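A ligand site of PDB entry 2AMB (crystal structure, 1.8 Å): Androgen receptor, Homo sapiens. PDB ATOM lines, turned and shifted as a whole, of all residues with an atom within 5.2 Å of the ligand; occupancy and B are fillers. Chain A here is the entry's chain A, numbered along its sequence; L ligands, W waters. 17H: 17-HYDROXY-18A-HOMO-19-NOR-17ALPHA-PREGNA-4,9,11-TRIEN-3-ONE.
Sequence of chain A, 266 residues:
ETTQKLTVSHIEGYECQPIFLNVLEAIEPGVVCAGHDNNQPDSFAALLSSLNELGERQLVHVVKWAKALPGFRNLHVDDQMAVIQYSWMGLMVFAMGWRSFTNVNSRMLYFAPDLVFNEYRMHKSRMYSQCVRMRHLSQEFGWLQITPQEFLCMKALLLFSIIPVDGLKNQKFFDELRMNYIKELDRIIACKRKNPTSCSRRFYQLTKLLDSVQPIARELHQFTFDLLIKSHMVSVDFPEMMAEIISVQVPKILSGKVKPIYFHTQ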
ATOM      1  N   LEU A  48     -21.271  -0.711   1.012  1.00  0.00           N
ATOM      2  CA  LEU A  48     -19.998  -0.038   0.845  1.00  0.00           C
ATOM      3  C   LEU A  48     -19.372   0.314   2.191  1.00  0.00           C
ATOM      4  O   LEU A  48     -18.148   0.259   2.334  1.00  0.00           O
ATOM      5  CB  LEU A  48     -20.137   1.134  -0.137  1.00  0.00           C
ATOM      6  CG  LEU A  48     -20.519   0.722  -1.589  1.00  0.00           C
ATOM      7  CD1 LEU A  48     -20.227   1.882  -2.510  1.00  0.00           C
ATOM      8  CD2 LEU A  48     -19.723  -0.501  -2.107  1.00  0.00           C
ATOM      9  N   LEU A  51     -17.818  -2.948   3.351  1.00  0.00           N
ATOM     10  CA  LEU A  51     -16.557  -3.254   2.617  1.00  0.00           C
ATOM     11  C   LEU A  51     -15.391  -2.425   3.149  1.00  0.00           C
ATOM     12  O   LEU A  51     -14.284  -2.948   3.333  1.00  0.00           O
ATOM     13  CB  LEU A  51     -16.660  -3.005   1.111  1.00  0.00           C
ATOM     14  CG  LEU A  51     -17.331  -4.127   0.279  1.00  0.00           C
ATOM     15  CD1 LEU A  51     -17.565  -3.631  -1.127  1.00  0.00           C
ATOM     16  CD2 LEU A  51     -16.421  -5.397   0.231  1.00  0.00           C
ATOM     17  N   ASN A  52     -15.643  -1.120   3.353  1.00  0.00           N
ATOM     18  CA  ASN A  52     -14.592  -0.220   3.861  1.00  0.00           C
ATOM     19  C   ASN A  52     -14.103  -0.665   5.227  1.00  0.00           C
ATOM     20  O   ASN A  52     -12.890  -0.638   5.514  1.00  0.00           O
ATOM     21  CB  ASN A  52     -15.088   1.241   3.905  1.00  0.00           C
ATOM     22  CG  ASN A  52     -14.990   1.925   2.546  1.00  0.00           C
ATOM     23  OD1 ASN A  52     -14.259   1.429   1.663  1.00  0.00           O
ATOM     24  ND2 ASN A  52     -15.672   3.076   2.360  1.00  0.00           N
ATOM     25  N   LEU A  54     -14.167  -3.752   6.397  1.00  0.00           N
ATOM     26  CA  LEU A  54     -13.394  -4.953   6.141  1.00  0.00           C
ATOM     27  C   LEU A  54     -12.003  -4.573   5.583  1.00  0.00           C
ATOM     28  O   LEU A  54     -11.000  -5.196   5.944  1.00  0.00           O
ATOM     29  CB  LEU A  54     -14.172  -5.857   5.139  1.00  0.00           C
ATOM     30  CG  LEU A  54     -13.414  -7.123   4.720  1.00  0.00           C
ATOM     31  CD1 LEU A  54     -13.180  -7.991   6.011  1.00  0.00           C
ATOM     32  CD2 LEU A  54     -14.217  -7.901   3.679  1.00  0.00           C
ATOM     33  N   GLY A  55     -11.956  -3.571   4.706  1.00  0.00           N
ATOM     34  CA  GLY A  55     -10.702  -3.112   4.138  1.00  0.00           C
ATOM     35  C   GLY A  55      -9.765  -2.658   5.247  1.00  0.00           C
ATOM     36  O   GLY A  55      -8.608  -2.962   5.216  1.00  0.00           O
ATOM     37  N   GLN A  58      -8.537  -5.797   7.095  1.00  0.00           N
ATOM     38  CA  GLN A  58      -7.588  -6.548   6.266  1.00  0.00           C
ATOM     39  C   GLN A  58      -6.197  -5.919   6.223  1.00  0.00           C
ATOM     40  O   GLN A  58      -5.154  -6.551   6.272  1.00  0.00           O
ATOM     41  CB  GLN A  58      -8.145  -6.636   4.847  1.00  0.00           C
ATOM     42  CG  GLN A  58      -9.115  -7.767   4.735  1.00  0.00           C
ATOM     43  CD  GLN A  58      -8.443  -9.057   5.060  1.00  0.00           C
ATOM     44  OE1 GLN A  58      -9.066 -10.031   5.454  1.00  0.00           O
ATOM     45  NE2 GLN A  58      -7.138  -9.087   4.883  1.00  0.00           N
ATOM     46  N   TRP A  88      -1.461  -2.906  -1.130  1.00  0.00           N
ATOM     47  CA  TRP A  88      -2.632  -3.318  -0.351  1.00  0.00           C
ATOM     48  C   TRP A  88      -3.843  -3.710  -1.183  1.00  0.00           C
ATOM     49  O   TRP A  88      -4.428  -4.792  -1.026  1.00  0.00           O
ATOM     50  CB  TRP A  88      -3.018  -2.199   0.638  1.00  0.00           C
ATOM     51  CG  TRP A  88      -4.390  -2.238   1.316  1.00  0.00           C
ATOM     52  CD1 TRP A  88      -4.939  -3.191   2.191  1.00  0.00           C
ATOM     53  CD2 TRP A  88      -5.294  -1.177   1.267  1.00  0.00           C
ATOM     54  NE1 TRP A  88      -6.146  -2.722   2.679  1.00  0.00           N
ATOM     55  CE2 TRP A  88      -6.390  -1.482   2.132  1.00  0.00           C
ATOM     56  CE3 TRP A  88      -5.288   0.050   0.574  1.00  0.00           C
ATOM     57  CZ2 TRP A  88      -7.460  -0.598   2.288  1.00  0.00           C
ATOM     58  CZ3 TRP A  88      -6.340   0.910   0.728  1.00  0.00           C
ATOM     59  CH2 TRP A  88      -7.414   0.597   1.579  1.00  0.00           C
ATOM     60  N   MET A  89      -4.229  -2.837  -2.118  1.00  0.00           N
ATOM     61  CA  MET A  89      -5.385  -3.126  -2.921  1.00  0.00           C
ATOM     62  C   MET A  89      -5.242  -4.445  -3.732  1.00  0.00           C
ATOM     63  O   MET A  89      -6.144  -5.332  -3.719  1.00  0.00           O
ATOM     64  CB  MET A  89      -5.656  -2.004  -3.958  1.00  0.00           C
ATOM     65  CG  MET A  89      -7.046  -2.236  -4.705  1.00  0.00           C
ATOM     66  SD  MET A  89      -8.505  -1.982  -3.629  1.00  0.00           S
ATOM     67  CE  MET A  89      -8.486  -0.172  -3.489  1.00  0.00           C
ATOM     68  N   MET A  92      -5.345  -7.528  -1.557  1.00  0.00           N
ATOM     69  CA  MET A  92      -6.684  -7.840  -1.062  1.00  0.00           C
ATOM     70  C   MET A  92      -7.485  -8.551  -2.122  1.00  0.00           C
ATOM     71  O   MET A  92      -8.114  -9.582  -1.842  1.00  0.00           O
ATOM     72  CB  MET A  92      -7.468  -6.590  -0.607  1.00  0.00           C
ATOM     73  CG  MET A  92      -6.897  -5.898   0.649  1.00  0.00           C
ATOM     74  SD  MET A  92      -8.168  -4.823   1.394  1.00  0.00           S
ATOM     75  CE  MET A  92      -8.486  -3.620   0.119  1.00  0.00           C
ATOM     76  N   VAL A  93      -7.390  -8.033  -3.344  1.00  0.00           N
ATOM     77  CA  VAL A  93      -8.112  -8.587  -4.487  1.00  0.00           C
ATOM     78  C   VAL A  93      -7.640 -10.011  -4.763  1.00  0.00           C
ATOM     79  O   VAL A  93      -8.487 -10.927  -5.027  1.00  0.00           O
ATOM     80  CB  VAL A  93      -7.856  -7.758  -5.747  1.00  0.00           C
ATOM     81  CG1 VAL A  93      -8.492  -8.476  -6.981  1.00  0.00           C
ATOM     82  CG2 VAL A  93      -8.510  -6.360  -5.588  1.00  0.00           C
ATOM     83  N   MET A  96      -8.759 -12.382  -2.069  1.00  0.00           N
ATOM     84  CA  MET A  96     -10.221 -12.508  -2.119  1.00  0.00           C
ATOM     85  C   MET A  96     -10.576 -13.442  -3.293  1.00  0.00           C
ATOM     86  O   MET A  96     -11.447 -14.325  -3.154  1.00  0.00           O
ATOM     87  CB  MET A  96     -10.889 -11.149  -2.273  1.00  0.00           C
ATOM     88  CG  MET A  96     -12.445 -11.226  -2.114  1.00  0.00           C
ATOM     89  SD  MET A  96     -13.261 -11.617  -3.705  1.00  0.00           S
ATOM     90  CE  MET A  96     -12.950 -10.047  -4.638  1.00  0.00           C
ATOM     91  N   ARG A  99      -9.938 -16.988  -2.015  1.00  0.00           N
ATOM     92  CA  ARG A  99     -11.006 -17.427  -1.090  1.00  0.00           C
ATOM     93  C   ARG A  99     -12.318 -17.785  -1.827  1.00  0.00           C
ATOM     94  O   ARG A  99     -13.012 -18.727  -1.438  1.00  0.00           O
ATOM     95  CB  ARG A  99     -11.360 -16.307  -0.081  1.00  0.00           C
ATOM     96  CG  ARG A  99     -10.330 -16.075   0.978  1.00  0.00           C
ATOM     97  CD  ARG A  99     -11.053 -15.297   2.101  1.00  0.00           C
ATOM     98  NE  ARG A  99     -11.421 -13.943   1.736  1.00  0.00           N
ATOM     99  CZ  ARG A  99     -10.571 -12.918   1.572  1.00  0.00           C
ATOM    100  NH1 ARG A  99      -9.255 -13.080   1.724  1.00  0.00           N
ATOM    101  NH2 ARG A  99     -11.071 -11.714   1.312  1.00  0.00           N
ATOM    102  N   PHE A 111     -15.770 -11.963   0.033  1.00  0.00           N
ATOM    103  CA  PHE A 111     -14.994 -10.925   0.705  1.00  0.00           C
ATOM    104  C   PHE A 111     -14.721 -11.337   2.140  1.00  0.00           C
ATOM    105  O   PHE A 111     -13.592 -11.150   2.658  1.00  0.00           O
ATOM    106  CB  PHE A 111     -15.763  -9.605   0.687  1.00  0.00           C
ATOM    107  CG  PHE A 111     -15.861  -8.962  -0.683  1.00  0.00           C
ATOM    108  CD1 PHE A 111     -17.078  -8.882  -1.356  1.00  0.00           C
ATOM    109  CD2 PHE A 111     -14.721  -8.394  -1.267  1.00  0.00           C
ATOM    110  CE1 PHE A 111     -17.192  -8.216  -2.640  1.00  0.00           C
ATOM    111  CE2 PHE A 111     -14.813  -7.729  -2.558  1.00  0.00           C
ATOM    112  CZ  PHE A 111     -16.054  -7.642  -3.231  1.00  0.00           C
ATOM    113  N   MET A 127     -20.852  -1.550  -7.937  1.00  0.00           N
ATOM    114  CA  MET A 127     -19.476  -1.946  -8.244  1.00  0.00           C
ATOM    115  C   MET A 127     -19.547  -3.137  -9.182  1.00  0.00           C
ATOM    116  O   MET A 127     -18.611  -3.951  -9.269  1.00  0.00           O
ATOM    117  CB  MET A 127     -18.756  -2.367  -6.952  1.00  0.00           C
ATOM    118  CG  MET A 127     -17.288  -2.193  -7.000  1.00  0.00           C
ATOM    119  SD  MET A 127     -16.660  -2.012  -5.333  1.00  0.00           S
ATOM    120  CE  MET A 127     -16.536  -3.742  -4.780  1.00  0.00           C
ATOM    121  N   MET A 134     -13.138  -8.936 -10.877  1.00  0.00           N
ATOM    122  CA  MET A 134     -12.596  -9.689  -9.780  1.00  0.00           C
ATOM    123  C   MET A 134     -13.012 -11.158  -9.819  1.00  0.00           C
ATOM    124  O   MET A 134     -12.209 -12.035  -9.509  1.00  0.00           O
ATOM    125  CB  MET A 134     -13.010  -9.043  -8.448  1.00  0.00           C
ATOM    126  CG  MET A 134     -12.250  -7.784  -8.174  1.00  0.00           C
ATOM    127  SD  MET A 134     -12.638  -7.060  -6.494  1.00  0.00           S
ATOM    128  CE  MET A 134     -14.192  -6.429  -6.680  1.00  0.00           C
ATOM    129  N   LEU A 220     -10.023  -0.430  -9.150  1.00  0.00           N
ATOM    130  CA  LEU A 220     -10.507  -0.304  -7.786  1.00  0.00           C
ATOM    131  C   LEU A 220      -9.928   0.951  -7.140  1.00  0.00           C
ATOM    132  O   LEU A 220     -10.600   1.568  -6.327  1.00  0.00           O
ATOM    133  CB  LEU A 220     -10.141  -1.554  -6.980  1.00  0.00           C
ATOM    134  CG  LEU A 220     -10.973  -2.785  -7.394  1.00  0.00           C
ATOM    135  CD1 LEU A 220     -10.442  -4.037  -6.698  1.00  0.00           C
ATOM    136  CD2 LEU A 220     -12.486  -2.562  -7.032  1.00  0.00           C
ATOM    137  N   PHE A 223     -12.020   3.688  -8.378  1.00  0.00           N
ATOM    138  CA  PHE A 223     -13.323   3.624  -7.730  1.00  0.00           C
ATOM    139  C   PHE A 223     -13.300   4.059  -6.263  1.00  0.00           C
ATOM    140  O   PHE A 223     -14.162   4.848  -5.859  1.00  0.00           O
ATOM    141  CB  PHE A 223     -13.906   2.191  -7.828  1.00  0.00           C
ATOM    142  CG  PHE A 223     -15.314   2.086  -7.306  1.00  0.00           C
ATOM    143  CD1 PHE A 223     -15.543   1.865  -5.933  1.00  0.00           C
ATOM    144  CD2 PHE A 223     -16.419   2.166  -8.158  1.00  0.00           C
ATOM    145  CE1 PHE A 223     -16.857   1.721  -5.435  1.00  0.00           C
ATOM    146  CE2 PHE A 223     -17.716   2.035  -7.695  1.00  0.00           C
ATOM    147  CZ  PHE A 223     -17.944   1.807  -6.330  1.00  0.00           C
ATOM    148  N   THR A 224     -12.329   3.642  -5.465  1.00  0.00           N
ATOM    149  CA  THR A 224     -12.332   4.020  -4.063  1.00  0.00           C
ATOM    150  C   THR A 224     -11.966   5.487  -3.924  1.00  0.00           C
ATOM    151  O   THR A 224     -12.477   6.200  -3.048  1.00  0.00           O
ATOM    152  CB  THR A 224     -11.383   3.097  -3.262  1.00  0.00           C
ATOM    153  OG1 THR A 224     -11.610   3.272  -1.867  1.00  0.00           O
ATOM    154  CG2 THR A 224      -9.938   3.411  -3.568  1.00  0.00           C
ATOM    155  N   LEU A 227     -15.017   7.521  -4.727  1.00  0.00           N
ATOM    156  CA  LEU A 227     -15.980   7.380  -3.634  1.00  0.00           C
ATOM    157  C   LEU A 227     -15.568   8.189  -2.401  1.00  0.00           C
ATOM    158  O   LEU A 227     -16.419   8.773  -1.697  1.00  0.00           O
ATOM    159  CB  LEU A 227     -16.126   5.895  -3.290  1.00  0.00           C
ATOM    160  CG  LEU A 227     -17.159   5.448  -2.253  1.00  0.00           C
ATOM    161  CD1 LEU A 227     -18.554   5.989  -2.565  1.00  0.00           C
ATOM    162  CD2 LEU A 227     -17.199   3.901  -2.280  1.00  0.00           C
ATOM    163  N   PHE A 238     -15.584   5.983   5.671  1.00  0.00           N
ATOM    164  CA  PHE A 238     -14.207   5.549   5.413  1.00  0.00           C
ATOM    165  C   PHE A 238     -13.394   5.646   6.721  1.00  0.00           C
ATOM    166  O   PHE A 238     -13.195   6.731   7.251  1.00  0.00           O
ATOM    167  CB  PHE A 238     -13.498   6.441   4.371  1.00  0.00           C
ATOM    168  CG  PHE A 238     -13.830   6.109   2.928  1.00  0.00           C
ATOM    169  CD1 PHE A 238     -15.026   6.522   2.354  1.00  0.00           C
ATOM    170  CD2 PHE A 238     -12.908   5.415   2.121  1.00  0.00           C
ATOM    171  CE1 PHE A 238     -15.324   6.257   0.982  1.00  0.00           C
ATOM    172  CE2 PHE A 238     -13.204   5.144   0.728  1.00  0.00           C
ATOM    173  CZ  PHE A 238     -14.400   5.556   0.182  1.00  0.00           C
ATOM    174  N   MET A 242      -7.370   5.081   6.122  1.00  0.00           N
ATOM    175  CA  MET A 242      -7.511   4.657   4.630  1.00  0.00           C
ATOM    176  C   MET A 242      -8.122   5.743   3.804  1.00  0.00           C
ATOM    177  O   MET A 242      -7.824   6.102   2.667  1.00  0.00           O
ATOM    178  CB  MET A 242      -8.441   3.535   4.588  1.00  0.00           C
ATOM    179  CG  MET A 242      -9.890   3.859   4.888  1.00  0.00           C
ATOM    180  SD  MET A 242     -10.862   2.591   4.144  1.00  0.00           S
ATOM    181  CE  MET A 242     -10.446   1.179   5.207  1.00  0.00           C
ATOM    182  N   ILE A 246      -5.776   6.411   0.820  1.00  0.00           N
ATOM    183  CA  ILE A 246      -6.513   6.708  -0.403  1.00  0.00           C
ATOM    184  C   ILE A 246      -6.285   8.154  -0.884  1.00  0.00           C
ATOM    185  O   ILE A 246      -6.277   8.432  -2.059  1.00  0.00           O
ATOM    186  CB  ILE A 246      -8.019   6.387  -0.202  1.00  0.00           C
ATOM    187  CG1 ILE A 246      -8.183   4.891   0.107  1.00  0.00           C
ATOM    188  CG2 ILE A 246      -8.861   6.838  -1.426  1.00  0.00           C
ATOM    189  CD1 ILE A 246      -9.564   4.466   0.530  1.00  0.00           C
HETATM  190  C2  17H L   1     -11.514  -6.917   1.402  1.00  0.00           C
HETATM  191  C4  17H L   1     -11.099  -7.448  -1.109  1.00  0.00           C
HETATM  192  C7  17H L   1     -12.211  -4.277  -2.959  1.00  0.00           C
HETATM  193  C6  17H L   1     -11.224  -5.437  -2.744  1.00  0.00           C
HETATM  194  C9  17H L   1     -12.108  -3.745  -0.487  1.00  0.00           C
HETATM  195  C11 17H L   1     -12.711  -2.806   0.573  1.00  0.00           C
HETATM  196  C1  17H L   1     -12.041  -5.619   1.174  1.00  0.00           C
HETATM  197  C3  17H L   1     -11.284  -7.752   0.239  1.00  0.00           C
HETATM  198  C5  17H L   1     -11.347  -6.071  -1.341  1.00  0.00           C
HETATM  199  C8  17H L   1     -11.926  -3.137  -1.935  1.00  0.00           C
HETATM  200  C10 17H L   1     -11.794  -5.097  -0.234  1.00  0.00           C
HETATM  201  C12 17H L   1     -13.111  -1.480   0.349  1.00  0.00           C
HETATM  202  C13 17H L   1     -12.903  -0.853  -0.999  1.00  0.00           C
HETATM  203  C14 17H L   1     -12.979  -1.998  -2.064  1.00  0.00           C
HETATM  204  C15 17H L   1     -13.048  -1.309  -3.440  1.00  0.00           C
HETATM  205  C16 17H L   1     -13.905  -0.063  -3.054  1.00  0.00           C
HETATM  206  C17 17H L   1     -14.001   0.063  -1.472  1.00  0.00           C
HETATM  207  C18 17H L   1     -11.359  -0.289  -1.054  1.00  0.00           C
HETATM  208  C22 17H L   1     -10.730   0.492   0.217  1.00  0.00           C
HETATM  209  C21 17H L   1     -16.363   0.885  -1.397  1.00  0.00           C
HETATM  210  C20 17H L   1     -15.422  -0.407  -1.141  1.00  0.00           C
HETATM  211  O3  17H L   1     -11.190  -9.132   0.560  1.00  0.00           O
HETATM  212  O17 17H L   1     -13.632   1.390  -1.025  1.00  0.00           O
HETATM  213  O   HOH W   1      -8.443 -10.188   0.917  1.00  0.00           O
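An oxygen (O17) of the ligand lies within hydrogen-bond range of the side-chain hydroxyl (OG1) of Thr 224, 2.9 Å away.
An oxygen (O17) of the ligand lies within hydrogen-bond range of the side-chain amide oxygen of Asn 52.
O3 of the ligand is in hydrogen-bond range of NH2 of Arg 99 (2.7 Å).
The side-chain sulfur (SD) of Met 92 sits at hydrogen-bond distance from the indole nitrogen (NE1) of Trp 88 (3.2 Å).
The backbone carbonyl oxygen of Phe 111 is in hydrogen-bond range of the guanidinium group of Arg 99 (2.9 Å).
CD2 of Leu 48 touches C21 of the ligand, 3.7 Å away.
Leu 51 touches the ligand.
Leu 54 touches the ligand (CD2 to C2, 3.7 Å).
Trp 88 touches the ligand (CH2 to C22, 3.6 Å).
CE of Met 89 touches C18 of the ligand, at 3.8 Å.
Met 92 touches the ligand.
Met 96 touches the ligand (CB to O3, 3.5 Å).
Phe 111 touches the ligand.
CD2 of Leu 220 touches C15 of the ligand, at 3.8 Å.
Phe 223 touches the ligand.
Leu 227 touches the ligand.
Hydrophobic or aromatic side chains that line the ligand: Leu 48, Leu 51, Leu 54, Trp 88, Met 89, Met 92, Met 96, Phe 111, Leu 220, Phe 223 and Leu 227.
Water W1 lies within hydrogen-bond range of the backbone carbonyl oxygen of Met 92 (2.8 Å), an oxygen (O3) of the ligand (3.0 Å) and the guanidinium group of Arg 99 (3.1 Å).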
